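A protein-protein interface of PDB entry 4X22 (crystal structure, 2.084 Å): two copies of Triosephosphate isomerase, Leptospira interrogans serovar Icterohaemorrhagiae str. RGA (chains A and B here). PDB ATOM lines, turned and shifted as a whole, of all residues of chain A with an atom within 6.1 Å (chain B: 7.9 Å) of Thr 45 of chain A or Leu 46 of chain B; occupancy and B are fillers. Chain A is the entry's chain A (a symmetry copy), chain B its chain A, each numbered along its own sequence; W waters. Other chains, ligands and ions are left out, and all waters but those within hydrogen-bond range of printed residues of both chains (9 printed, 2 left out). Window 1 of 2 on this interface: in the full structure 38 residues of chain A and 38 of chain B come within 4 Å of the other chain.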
ATOM      1  N   PRO A  43      19.488  -0.955   2.841  1.00  0.00           N
ATOM      2  CA  PRO A  43      20.348  -1.771   3.672  1.00  0.00           C
ATOM      3  C   PRO A  43      19.979  -3.251   3.750  1.00  0.00           C
ATOM      4  O   PRO A  43      18.837  -3.630   3.464  1.00  0.00           O
ATOM      5  CB  PRO A  43      20.272  -1.097   5.083  1.00  0.00           C
ATOM      6  CG  PRO A  43      19.418   0.117   4.903  1.00  0.00           C
ATOM      7  CD  PRO A  43      18.599  -0.097   3.651  1.00  0.00           C
ATOM      8  N   SER A  44      20.943  -4.070   4.155  1.00  0.00           N
ATOM      9  CA  SER A  44      20.674  -5.488   4.463  1.00  0.00           C
ATOM     10  C   SER A  44      19.605  -5.498   5.562  1.00  0.00           C
ATOM     11  O   SER A  44      19.554  -4.629   6.475  1.00  0.00           O
ATOM     12  CB  SER A  44      21.918  -6.198   4.923  1.00  0.00           C
ATOM     13  OG  SER A  44      22.883  -6.289   3.867  1.00  0.00           O
ATOM     14  N   THR A  45      18.771  -6.502   5.509  1.00  0.00           N
ATOM     15  CA  THR A  45      17.686  -6.673   6.499  1.00  0.00           C
ATOM     16  C   THR A  45      18.141  -6.746   7.919  1.00  0.00           C
ATOM     17  O   THR A  45      17.508  -6.160   8.791  1.00  0.00           O
ATOM     18  CB  THR A  45      16.820  -7.890   6.084  1.00  0.00           C
ATOM     19  OG1 THR A  45      16.194  -7.529   4.809  1.00  0.00           O
ATOM     20  CG2 THR A  45      15.821  -8.230   7.154  1.00  0.00           C
ATOM     21  N   LEU A  46      19.285  -7.355   8.159  1.00  0.00           N
ATOM     22  CA  LEU A  46      19.880  -7.435   9.495  1.00  0.00           C
ATOM     23  C   LEU A  46      20.159  -6.017  10.103  1.00  0.00           C
ATOM     24  O   LEU A  46      20.152  -5.786  11.335  1.00  0.00           O
ATOM     25  CB  LEU A  46      21.210  -8.210   9.423  1.00  0.00           C
ATOM     26  CG  LEU A  46      21.752  -8.617  10.781  1.00  0.00           C
ATOM     27  CD1 LEU A  46      21.000  -9.790  11.343  1.00  0.00           C
ATOM     28  CD2 LEU A  46      23.171  -9.088  10.594  1.00  0.00           C
ATOM     29  N   HIS A  47      20.441  -5.091   9.213  1.00  0.00           N
ATOM     30  CA  HIS A  47      20.743  -3.725   9.572  1.00  0.00           C
ATOM     31  C   HIS A  47      19.625  -2.688   9.478  1.00  0.00           C
ATOM     32  O   HIS A  47      19.819  -1.497   9.842  1.00  0.00           O
ATOM     33  CB  HIS A  47      21.889  -3.232   8.669  1.00  0.00           C
ATOM     34  CG  HIS A  47      23.054  -4.119   8.632  1.00  0.00           C
ATOM     35  ND1 HIS A  47      23.949  -4.123   7.586  1.00  0.00           N
ATOM     36  CD2 HIS A  47      23.513  -5.011   9.530  1.00  0.00           C
ATOM     37  CE1 HIS A  47      24.912  -4.976   7.854  1.00  0.00           C
ATOM     38  NE2 HIS A  47      24.663  -5.534   9.024  1.00  0.00           N
ATOM     39  N   LEU A  48      18.424  -3.110   9.046  1.00  0.00           N
ATOM     40  CA  LEU A  48      17.392  -2.179   8.720  1.00  0.00           C
ATOM     41  C   LEU A  48      16.871  -1.410   9.918  1.00  0.00           C
ATOM     42  O   LEU A  48      16.550  -0.240   9.806  1.00  0.00           O
ATOM     43  CB  LEU A  48      16.198  -2.839   8.041  1.00  0.00           C
ATOM     44  CG  LEU A  48      16.271  -3.135   6.542  1.00  0.00           C
ATOM     45  CD1 LEU A  48      15.005  -3.937   6.147  1.00  0.00           C
ATOM     46  CD2 LEU A  48      16.298  -1.753   5.896  1.00  0.00           C
ATOM     47  N   GLU A  49      16.731  -2.075  11.038  1.00  0.00           N
ATOM     48  CA  GLU A  49      16.207  -1.441  12.213  1.00  0.00           C
ATOM     49  C   GLU A  49      17.092  -0.294  12.668  1.00  0.00           C
ATOM     50  O   GLU A  49      16.677   0.759  12.962  1.00  0.00           O
ATOM     51  CB  GLU A  49      16.063  -2.443  13.306  1.00  0.00           C
ATOM     52  CG  GLU A  49      15.019  -2.003  14.277  1.00  0.00           C
ATOM     53  CD  GLU A  49      15.517  -2.019  15.645  1.00  0.00           C
ATOM     54  OE1 GLU A  49      15.658  -3.088  16.223  1.00  0.00           O
ATOM     55  OE2 GLU A  49      15.805  -0.972  16.106  1.00  0.00           O
ATOM     56  N   ALA A  64      13.586  -2.100   2.000  1.00  0.00           N
ATOM     57  CA  ALA A  64      14.082  -3.477   2.130  1.00  0.00           C
ATOM     58  C   ALA A  64      14.431  -4.101   0.770  1.00  0.00           C
ATOM     59  O   ALA A  64      13.806  -3.804  -0.241  1.00  0.00           O
ATOM     60  CB  ALA A  64      13.081  -4.350   2.834  1.00  0.00           C
ATOM     61  N   GLN A  65      15.497  -4.905   0.764  1.00  0.00           N
ATOM     62  CA  GLN A  65      15.947  -5.591  -0.418  1.00  0.00           C
ATOM     63  C   GLN A  65      15.049  -6.778  -0.870  1.00  0.00           C
ATOM     64  O   GLN A  65      15.189  -7.288  -2.026  1.00  0.00           O
ATOM     65  CB  GLN A  65      17.391  -6.076  -0.220  1.00  0.00           C
ATOM     66  CG  GLN A  65      18.409  -4.966  -0.073  1.00  0.00           C
ATOM     67  CD  GLN A  65      19.794  -5.494   0.272  1.00  0.00           C
ATOM     68  OE1 GLN A  65      20.090  -6.670   0.065  1.00  0.00           O
ATOM     69  NE2 GLN A  65      20.650  -4.630   0.766  1.00  0.00           N
ATOM     70  N   ASN A  66      14.143  -7.218   0.000  1.00  0.00           N
ATOM     71  CA  ASN A  66      13.270  -8.334  -0.348  1.00  0.00           C
ATOM     72  C   ASN A  66      12.243  -8.505   0.797  1.00  0.00           C
ATOM     73  O   ASN A  66      12.461  -8.010   1.910  1.00  0.00           O
ATOM     74  CB  ASN A  66      14.117  -9.633  -0.435  1.00  0.00           C
ATOM     75  CG  ASN A  66      13.270 -10.817  -0.817  1.00  0.00           C
ATOM     76  OD1 ASN A  66      12.480 -10.719  -1.733  1.00  0.00           O
ATOM     77  ND2 ASN A  66      13.416 -11.904  -0.125  1.00  0.00           N
ATOM     78  N   THR A  79      10.912 -12.300   5.798  1.00  0.00           N
ATOM     79  CA  THR A  79      10.557 -11.048   6.444  1.00  0.00           C
ATOM     80  C   THR A  79       9.156 -10.577   5.946  1.00  0.00           C
ATOM     81  O   THR A  79       8.841 -10.588   4.756  1.00  0.00           O
ATOM     82  CB  THR A  79      11.587  -9.973   6.035  1.00  0.00           C
ATOM     83  OG1 THR A  79      12.914 -10.345   6.474  1.00  0.00           O
ATOM     84  CG2 THR A  79      11.266  -8.622   6.636  1.00  0.00           C
ATOM     85  N   SER A  80       8.313 -10.140   6.856  1.00  0.00           N
ATOM     86  CA  SER A  80       6.969  -9.723   6.527  1.00  0.00           C
ATOM     87  C   SER A  80       6.892  -8.208   6.331  1.00  0.00           C
ATOM     88  O   SER A  80       7.533  -7.425   7.097  1.00  0.00           O
ATOM     89  CB  SER A  80       6.008 -10.043   7.655  1.00  0.00           C
ATOM     90  OG  SER A  80       4.650  -9.582   7.357  1.00  0.00           O
ATOM     91  N   GLN A  83       6.371  -6.598   9.625  1.00  0.00           N
ATOM     92  CA  GLN A  83       7.585  -6.267  10.381  1.00  0.00           C
ATOM     93  C   GLN A  83       8.278  -4.991   9.889  1.00  0.00           C
ATOM     94  O   GLN A  83       8.815  -4.171  10.706  1.00  0.00           O
ATOM     95  CB  GLN A  83       8.547  -7.445  10.367  1.00  0.00           C
ATOM     96  CG  GLN A  83       7.950  -8.694  10.969  1.00  0.00           C
ATOM     97  CD  GLN A  83       8.811  -9.903  10.760  1.00  0.00           C
ATOM     98  OE1 GLN A  83       9.328 -10.169   9.643  1.00  0.00           O
ATOM     99  NE2 GLN A  83       8.921 -10.690  11.784  1.00  0.00           N
ATOM    100  N   LEU A  84       8.314  -4.812   8.568  1.00  0.00           N
ATOM    101  CA  LEU A  84       8.925  -3.606   7.975  1.00  0.00           C
ATOM    102  C   LEU A  84       8.156  -2.318   8.340  1.00  0.00           C
ATOM    103  O   LEU A  84       8.772  -1.292   8.715  1.00  0.00           O
ATOM    104  CB  LEU A  84       8.977  -3.740   6.429  1.00  0.00           C
ATOM    105  CG  LEU A  84       9.877  -4.915   6.003  1.00  0.00           C
ATOM    106  CD1 LEU A  84       9.775  -5.176   4.536  1.00  0.00           C
ATOM    107  CD2 LEU A  84      11.359  -4.688   6.333  1.00  0.00           C
ATOM    108  N   ILE A  87       8.854  -0.695  11.739  1.00  0.00           N
ATOM    109  CA  ILE A  87      10.020   0.117  11.913  1.00  0.00           C
ATOM    110  C   ILE A  87      10.099   1.236  10.900  1.00  0.00           C
ATOM    111  O   ILE A  87      11.151   1.766  10.730  1.00  0.00           O
ATOM    112  CB  ILE A  87      11.342  -0.716  11.855  1.00  0.00           C
ATOM    113  CG1 ILE A  87      11.446  -1.509  10.528  1.00  0.00           C
ATOM    114  CG2 ILE A  87      11.355  -1.768  12.948  1.00  0.00           C
ATOM    115  CD1 ILE A  87      12.833  -2.075  10.233  1.00  0.00           C
ATOM    116  N   LEU B  14       6.329 -12.944  14.781  1.00  0.00           N
ATOM    117  CA  LEU B  14       6.391 -11.887  15.809  1.00  0.00           C
ATOM    118  C   LEU B  14       6.725 -10.481  15.304  1.00  0.00           C
ATOM    119  O   LEU B  14       7.531 -10.282  14.362  1.00  0.00           O
ATOM    120  CB  LEU B  14       7.441 -12.246  16.841  1.00  0.00           C
ATOM    121  CG  LEU B  14       7.253 -13.573  17.543  1.00  0.00           C
ATOM    122  CD1 LEU B  14       8.257 -13.777  18.644  1.00  0.00           C
ATOM    123  CD2 LEU B  14       5.851 -13.667  18.118  1.00  0.00           C
ATOM    124  N   SER B  15       6.100  -9.492  15.932  1.00  0.00           N
ATOM    125  CA  SER B  15       6.467  -8.107  15.758  1.00  0.00           C
ATOM    126  C   SER B  15       7.767  -7.872  16.491  1.00  0.00           C
ATOM    127  O   SER B  15       8.193  -8.706  17.333  1.00  0.00           O
ATOM    128  CB  SER B  15       5.388  -7.186  16.361  1.00  0.00           C
ATOM    129  OG  SER B  15       5.386  -7.400  17.762  1.00  0.00           O
ATOM    130  N   LEU B  16       8.427  -6.756  16.198  1.00  0.00           N
ATOM    131  CA  LEU B  16       9.643  -6.437  16.898  1.00  0.00           C
ATOM    132  C   LEU B  16       9.343  -6.226  18.431  1.00  0.00           C
ATOM    133  O   LEU B  16      10.057  -6.689  19.299  1.00  0.00           O
ATOM    134  CB  LEU B  16      10.254  -5.179  16.354  1.00  0.00           C
ATOM    135  CG  LEU B  16      11.454  -4.608  17.147  1.00  0.00           C
ATOM    136  CD1 LEU B  16      12.642  -5.580  17.298  1.00  0.00           C
ATOM    137  CD2 LEU B  16      11.854  -3.265  16.573  1.00  0.00           C
ATOM    138  N   ALA B  19       9.017  -9.591  19.882  1.00  0.00           N
ATOM    139  CA  ALA B  19      10.338 -10.246  19.967  1.00  0.00           C
ATOM    140  C   ALA B  19      11.163  -9.730  21.133  1.00  0.00           C
ATOM    141  O   ALA B  19      11.874 -10.499  21.785  1.00  0.00           O
ATOM    142  CB  ALA B  19      11.114 -10.042  18.665  1.00  0.00           C
ATOM    143  N   PRO B  43      15.103 -15.798  16.259  1.00  0.00           N
ATOM    144  CA  PRO B  43      14.333 -14.652  15.822  1.00  0.00           C
ATOM    145  C   PRO B  43      14.377 -14.360  14.324  1.00  0.00           C
ATOM    146  O   PRO B  43      15.292 -14.806  13.622  1.00  0.00           O
ATOM    147  CB  PRO B  43      14.921 -13.457  16.646  1.00  0.00           C
ATOM    148  CG  PRO B  43      15.943 -14.060  17.557  1.00  0.00           C
ATOM    149  CD  PRO B  43      16.338 -15.391  16.960  1.00  0.00           C
ATOM    150  N   SER B  44      13.397 -13.597  13.851  1.00  0.00           N
ATOM    151  CA  SER B  44      13.421 -13.076  12.471  1.00  0.00           C
ATOM    152  C   SER B  44      14.711 -12.259  12.337  1.00  0.00           C
ATOM    153  O   SER B  44      15.187 -11.573  13.283  1.00  0.00           O
ATOM    154  CB  SER B  44      12.216 -12.222  12.184  1.00  0.00           C
ATOM    155  OG  SER B  44      11.013 -13.000  12.200  1.00  0.00           O
ATOM    156  N   THR B  45      15.261 -12.289  11.153  1.00  0.00           N
ATOM    157  CA  THR B  45      16.503 -11.547  10.846  1.00  0.00           C
ATOM    158  C   THR B  45      16.431 -10.077  11.097  1.00  0.00           C
ATOM    159  O   THR B  45      17.382  -9.501  11.614  1.00  0.00           O
ATOM    160  CB  THR B  45      16.942 -11.888   9.400  1.00  0.00           C
ATOM    161  OG1 THR B  45      17.276 -13.314   9.400  1.00  0.00           O
ATOM    162  CG2 THR B  45      18.087 -11.016   8.965  1.00  0.00           C
ATOM    163  N   LEU B  46      15.284  -9.475  10.849  1.00  0.00           N
ATOM    164  CA  LEU B  46      15.057  -8.052  11.117  1.00  0.00           C
ATOM    165  C   LEU B  46      15.264  -7.698  12.630  1.00  0.00           C
ATOM    166  O   LEU B  46      15.643  -6.569  13.023  1.00  0.00           O
ATOM    167  CB  LEU B  46      13.618  -7.675  10.715  1.00  0.00           C
ATOM    168  CG  LEU B  46      13.375  -6.178  10.660  1.00  0.00           C
ATOM    169  CD1 LEU B  46      13.973  -5.569   9.423  1.00  0.00           C
ATOM    170  CD2 LEU B  46      11.890  -5.951  10.556  1.00  0.00           C
ATOM    171  N   HIS B  47      14.969  -8.672  13.463  1.00  0.00           N
ATOM    172  CA  HIS B  47      15.078  -8.539  14.896  1.00  0.00           C
ATOM    173  C   HIS B  47      16.330  -9.082  15.580  1.00  0.00           C
ATOM    174  O   HIS B  47      16.504  -8.931  16.819  1.00  0.00           O
ATOM    175  CB  HIS B  47      13.872  -9.250  15.538  1.00  0.00           C
ATOM    176  CG  HIS B  47      12.573  -8.851  14.991  1.00  0.00           C
ATOM    177  ND1 HIS B  47      11.457  -9.654  15.074  1.00  0.00           N
ATOM    178  CD2 HIS B  47      12.181  -7.713  14.387  1.00  0.00           C
ATOM    179  CE1 HIS B  47      10.436  -9.015  14.549  1.00  0.00           C
ATOM    180  NE2 HIS B  47      10.854  -7.840  14.116  1.00  0.00           N
ATOM    181  N   LEU B  48      17.254  -9.672  14.802  1.00  0.00           N
ATOM    182  CA  LEU B  48      18.344 -10.397  15.375  1.00  0.00           C
ATOM    183  C   LEU B  48      19.315  -9.522  16.142  1.00  0.00           C
ATOM    184  O   LEU B  48      19.843  -9.935  17.160  1.00  0.00           O
ATOM    185  CB  LEU B  48      19.143 -11.173  14.336  1.00  0.00           C
ATOM    186  CG  LEU B  48      18.618 -12.528  13.860  1.00  0.00           C
ATOM    187  CD1 LEU B  48      19.529 -13.021  12.707  1.00  0.00           C
ATOM    188  CD2 LEU B  48      18.727 -13.419  15.096  1.00  0.00           C
ATOM    189  N   GLU B  49      19.593  -8.350  15.629  1.00  0.00           N
ATOM    190  CA  GLU B  49      20.532  -7.470  16.264  1.00  0.00           C
ATOM    191  C   GLU B  49      20.070  -7.073  17.655  1.00  0.00           C
ATOM    192  O   GLU B  49      20.767  -7.095  18.593  1.00  0.00           O
ATOM    193  CB  GLU B  49      20.734  -6.256  15.425  1.00  0.00           C
ATOM    194  CG  GLU B  49      22.066  -5.646  15.708  1.00  0.00           C
ATOM    195  CD  GLU B  49      21.952  -4.228  16.017  1.00  0.00           C
ATOM    196  OE1 GLU B  49      21.736  -3.429  15.115  1.00  0.00           O
ATOM    197  OE2 GLU B  49      22.031  -3.936  17.158  1.00  0.00           O
ATOM    198  N   ASN B  50      18.820  -6.742  17.698  1.00  0.00           N
ATOM    199  CA  ASN B  50      18.161  -6.344  18.882  1.00  0.00           C
ATOM    200  C   ASN B  50      18.141  -7.422  19.979  1.00  0.00           C
ATOM    201  O   ASN B  50      18.574  -7.208  21.084  1.00  0.00           O
ATOM    202  CB  ASN B  50      16.777  -5.966  18.474  1.00  0.00           C
ATOM    203  CG  ASN B  50      16.294  -4.797  19.202  1.00  0.00           C
ATOM    204  OD1 ASN B  50      15.882  -4.875  20.341  1.00  0.00           O
ATOM    205  ND2 ASN B  50      16.276  -3.702  18.519  1.00  0.00           N
ATOM    206  N   VAL B  51      17.629  -8.576  19.594  1.00  0.00           N
ATOM    207  CA  VAL B  51      17.501  -9.739  20.418  1.00  0.00           C
ATOM    208  C   VAL B  51      18.863 -10.206  20.881  1.00  0.00           C
ATOM    209  O   VAL B  51      19.014 -10.488  22.008  1.00  0.00           O
ATOM    210  CB  VAL B  51      16.679 -10.895  19.792  1.00  0.00           C
ATOM    211  CG1 VAL B  51      16.817 -12.168  20.590  1.00  0.00           C
ATOM    212  CG2 VAL B  51      15.227 -10.516  19.589  1.00  0.00           C
ATOM    213  N   GLY B  77      19.251  -9.007  -1.026  1.00  0.00           N
ATOM    214  CA  GLY B  77      18.247  -9.721  -0.235  1.00  0.00           C
ATOM    215  C   GLY B  77      18.727 -10.785   0.725  1.00  0.00           C
ATOM    216  O   GLY B  77      17.922 -11.299   1.535  1.00  0.00           O
ATOM    217  N   GLU B  78      20.014 -11.130   0.648  1.00  0.00           N
ATOM    218  CA  GLU B  78      20.561 -12.260   1.408  1.00  0.00           C
ATOM    219  C   GLU B  78      21.319 -11.716   2.620  1.00  0.00           C
ATOM    220  O   GLU B  78      21.773 -10.595   2.622  1.00  0.00           O
ATOM    221  CB  GLU B  78      21.492 -13.145   0.566  1.00  0.00           C
ATOM    222  CG  GLU B  78      20.726 -13.922  -0.516  1.00  0.00           C
ATOM    223  CD  GLU B  78      19.622 -14.823   0.106  1.00  0.00           C
ATOM    224  OE1 GLU B  78      19.988 -15.786   0.804  1.00  0.00           O
ATOM    225  OE2 GLU B  78      18.423 -14.545  -0.101  1.00  0.00           O
ATOM    226  N   THR B  79      21.456 -12.564   3.603  1.00  0.00           N
ATOM    227  CA  THR B  79      22.233 -12.278   4.797  1.00  0.00           C
ATOM    228  C   THR B  79      23.523 -13.154   4.810  1.00  0.00           C
ATOM    229  O   THR B  79      23.505 -14.357   4.548  1.00  0.00           O
ATOM    230  CB  THR B  79      21.393 -12.659   6.034  1.00  0.00           C
ATOM    231  OG1 THR B  79      20.178 -11.874   6.089  1.00  0.00           O
ATOM    232  CG2 THR B  79      22.147 -12.428   7.326  1.00  0.00           C
ATOM    233  N   GLN B  83      27.973 -11.053   8.401  1.00  0.00           N
ATOM    234  CA  GLN B  83      27.103 -10.132   9.143  1.00  0.00           C
ATOM    235  C   GLN B  83      26.602 -10.708  10.471  1.00  0.00           C
ATOM    236  O   GLN B  83      26.490  -9.976  11.510  1.00  0.00           O
ATOM    237  CB  GLN B  83      25.937  -9.698   8.267  1.00  0.00           C
ATOM    238  CG  GLN B  83      26.382  -9.002   7.003  1.00  0.00           C
ATOM    239  CD  GLN B  83      25.254  -8.770   6.044  1.00  0.00           C
ATOM    240  OE1 GLN B  83      24.418  -9.669   5.768  1.00  0.00           O
ATOM    241  NE2 GLN B  83      25.246  -7.609   5.466  1.00  0.00           N
HETATM  242  O   HOH W   1      21.339  -8.042   2.092  1.00  0.00           O
HETATM  243  O   HOH W   2      16.415  -9.028   2.410  1.00  0.00           O
HETATM  244  O   HOH W   3      13.312 -10.682   9.136  1.00  0.00           O
HETATM  245  O   HOH W   4       9.392  -5.566  13.042  1.00  0.00           O
HETATM  246  O   HOH W   5      17.166  -5.835  15.313  1.00  0.00           O
HETATM  247  O   HOH W   6      26.254  -7.338  10.660  1.00  0.00           O
HETATM  248  O   HOH W   7      19.481  -3.415  12.759  1.00  0.00           O
HETATM  249  O   HOH W   8      20.427  -9.178   6.249  1.00  0.00           O
HETATM  250  O   HOH W   9      14.765 -11.841   2.485  1.00  0.00           O
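The backbone carbonyl oxygen (O) of Leu 14 of chain B is in hydrogen-bond range of the side-chain amide nitrogen (NE2) of Gln 83 of chain A (3.0 Å). The side-chain amide nitrogen (NE2) of Gln 83 of chain A is in hydrogen-bond range of the side-chain hydroxyl (OG) of Ser 44 of chain B, 3.1 Å away. The side-chain amide nitrogen (ND2) of Asn 50 of chain B is in hydrogen-bond range of the side-chain carboxylate (OE1) of Glu 49 of chain A, at 2.5 Å. The side-chain amide oxygen (OE1) of Gln 65 of chain A is in hydrogen-bond range of the backbone NH (N) of Gly 77 of chain B (2.7 Å). The side-chain hydroxyl (OG) of Ser 44 of chain A is in hydrogen-bond range of the side-chain amide nitrogen (NE2) of Gln 83 of chain B.
The backbone NH of Leu 16 of chain B lies close to a ring nitrogen (NE2) of His 47 of chain B, at 3.4 Å. NE2 of Gln 65 of chain A sits close to O of Pro 43 of chain A (3.4 Å). N of Ser 44 of chain A lies close to NE2 of Gln 65 of chain A (3.4 Å). The side-chain amide oxygen (OE1) of Gln 83 of chain A is in hydrogen-bond range of the backbone NH (N) of Ser 80 of chain A (3.0 Å).
Among the printed residues, pairs that only touch across the chains: Thr 45 of chain A with Leu 46 of chain B (3.6 Å), Leu 46 of chain A with Thr 45 of chain B (3.6 Å), Leu 46 of chain A with Leu 48 of chain B (3.8 Å), Leu 46 of chain A with Gln 83 of chain B (3.6 Å), His 47 of chain A with Gln 83 of chain B (3.6 Å), Leu 48 of chain A with Leu 46 of chain B (3.8 Å), Glu 49 of chain A with Leu 16 of chain B (3.8 Å), Gln 83 of chain A with Leu 46 of chain B (3.6 Å), Gln 83 of chain A with His 47 of chain B (3.6 Å), Ile 87 of chain A with Leu 16 of chain B (3.95 Å) and Ile 87 of chain A with Leu 46 of chain B (3.8 Å).
Pro 43 of chain A touches none of the printed residues of chain B. Printed residues of chain B within 4 Å of Ser 44 of chain A: Gln 83 (3.1 Å). Thr 45 of chain A touches one residue of chain B. Ser 80 of chain A touches none of the printed residues of chain B. Leu 46 of chain B touches four residues of chain A. Of the printed residues of chain A, Leu 48 of chain B touches Leu 46 (3.8 Å). Printed residues of chain A within 4 Å of Gln 83 of chain B: Ser 44, Leu 46 and His 47. The nearest printed residue of chain B that does not touch Ser 44 of chain A is Glu 78 of chain B (4.6 Å).
Of the 15 printed residues of chain A, 9 touch a printed residue of chain B. Printed residues of chain A that touch a printed residue of chain B: Ser 44, Thr 45, Leu 46, His 47, Leu 48, Glu 49, Gln 65, Gln 83 and Ile 87. Hydrophobic or aromatic side chains of chain A that line the printed part of chain B: Leu 46, His 47, Leu 48 and Ile 87. Printed residues of chain B that touch a printed residue of chain A: Leu 14, Leu 16, Ser 44, Thr 45, Leu 46, His 47, Leu 48, Asn 50, Gly 77 and Gln 83. Hydrophobic or aromatic side chains of chain B within 4 Å of the printed part of chain A: Leu 16, Leu 46, His 47 and Leu 48.
Ser 44 of chain A touches Gln 83 of chain B, and with the chains exchanged Gln 83 of chain A touches Ser 44 of chain B. Thr 45 of chain A touches Leu 46 of chain B, and with the chains exchanged Leu 46 of chain A touches Thr 45 of chain B. Leu 46 of chain A touches Leu 48 of chain B, and with the chains exchanged Leu 48 of chain A touches Leu 46 of chain B. Leu 46 of chain A touches Gln 83 of chain B, and with the chains exchanged Gln 83 of chain A touches Leu 46 of chain B. Positions printed for both chains: 43, 44, 45, 46, 47, 48, 49, 79 and 83.
Water W1 lies within hydrogen-bond range of O of Glu 78 of chain B (2.6 Å), OE1 of Gln 65 of chain A (2.7 Å) and OG of Ser 44 of chain A (2.9 Å). Water W8 lies within hydrogen-bond range of OG1 of Thr 79 of chain B (2.7 Å), N of Leu 46 of chain A (2.9 Å) and N of Thr 45 of chain A (3.2 Å). Water W3 lies within hydrogen-bond range of the side-chain hydroxyl (OG1) of Thr 79 of chain A (2.7 Å), the backbone NH (N) of Leu 46 of chain B (2.9 Å) and the backbone NH (N) of Thr 45 of chain B (3.2 Å). Water W2 lies within hydrogen-bond range of the side-chain hydroxyl (OG1) of Thr 45 of chain A (2.8 Å) and the backbone carbonyl oxygen (O) of Gly 77 of chain B (2.9 Å). Water W7 lies within hydrogen-bond range of O of Leu 46 of chain A and OE1 of Glu 49 of chain B. Water W5 lies within hydrogen-bond range of the backbone carbonyl oxygen (O) of Leu 46 of chain B (2.8 Å), the backbone NH (N) of Asn 50 of chain B (3.0 Å) and the side-chain carboxylate (OE1) of Glu 49 of chain A (3.3 Å).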
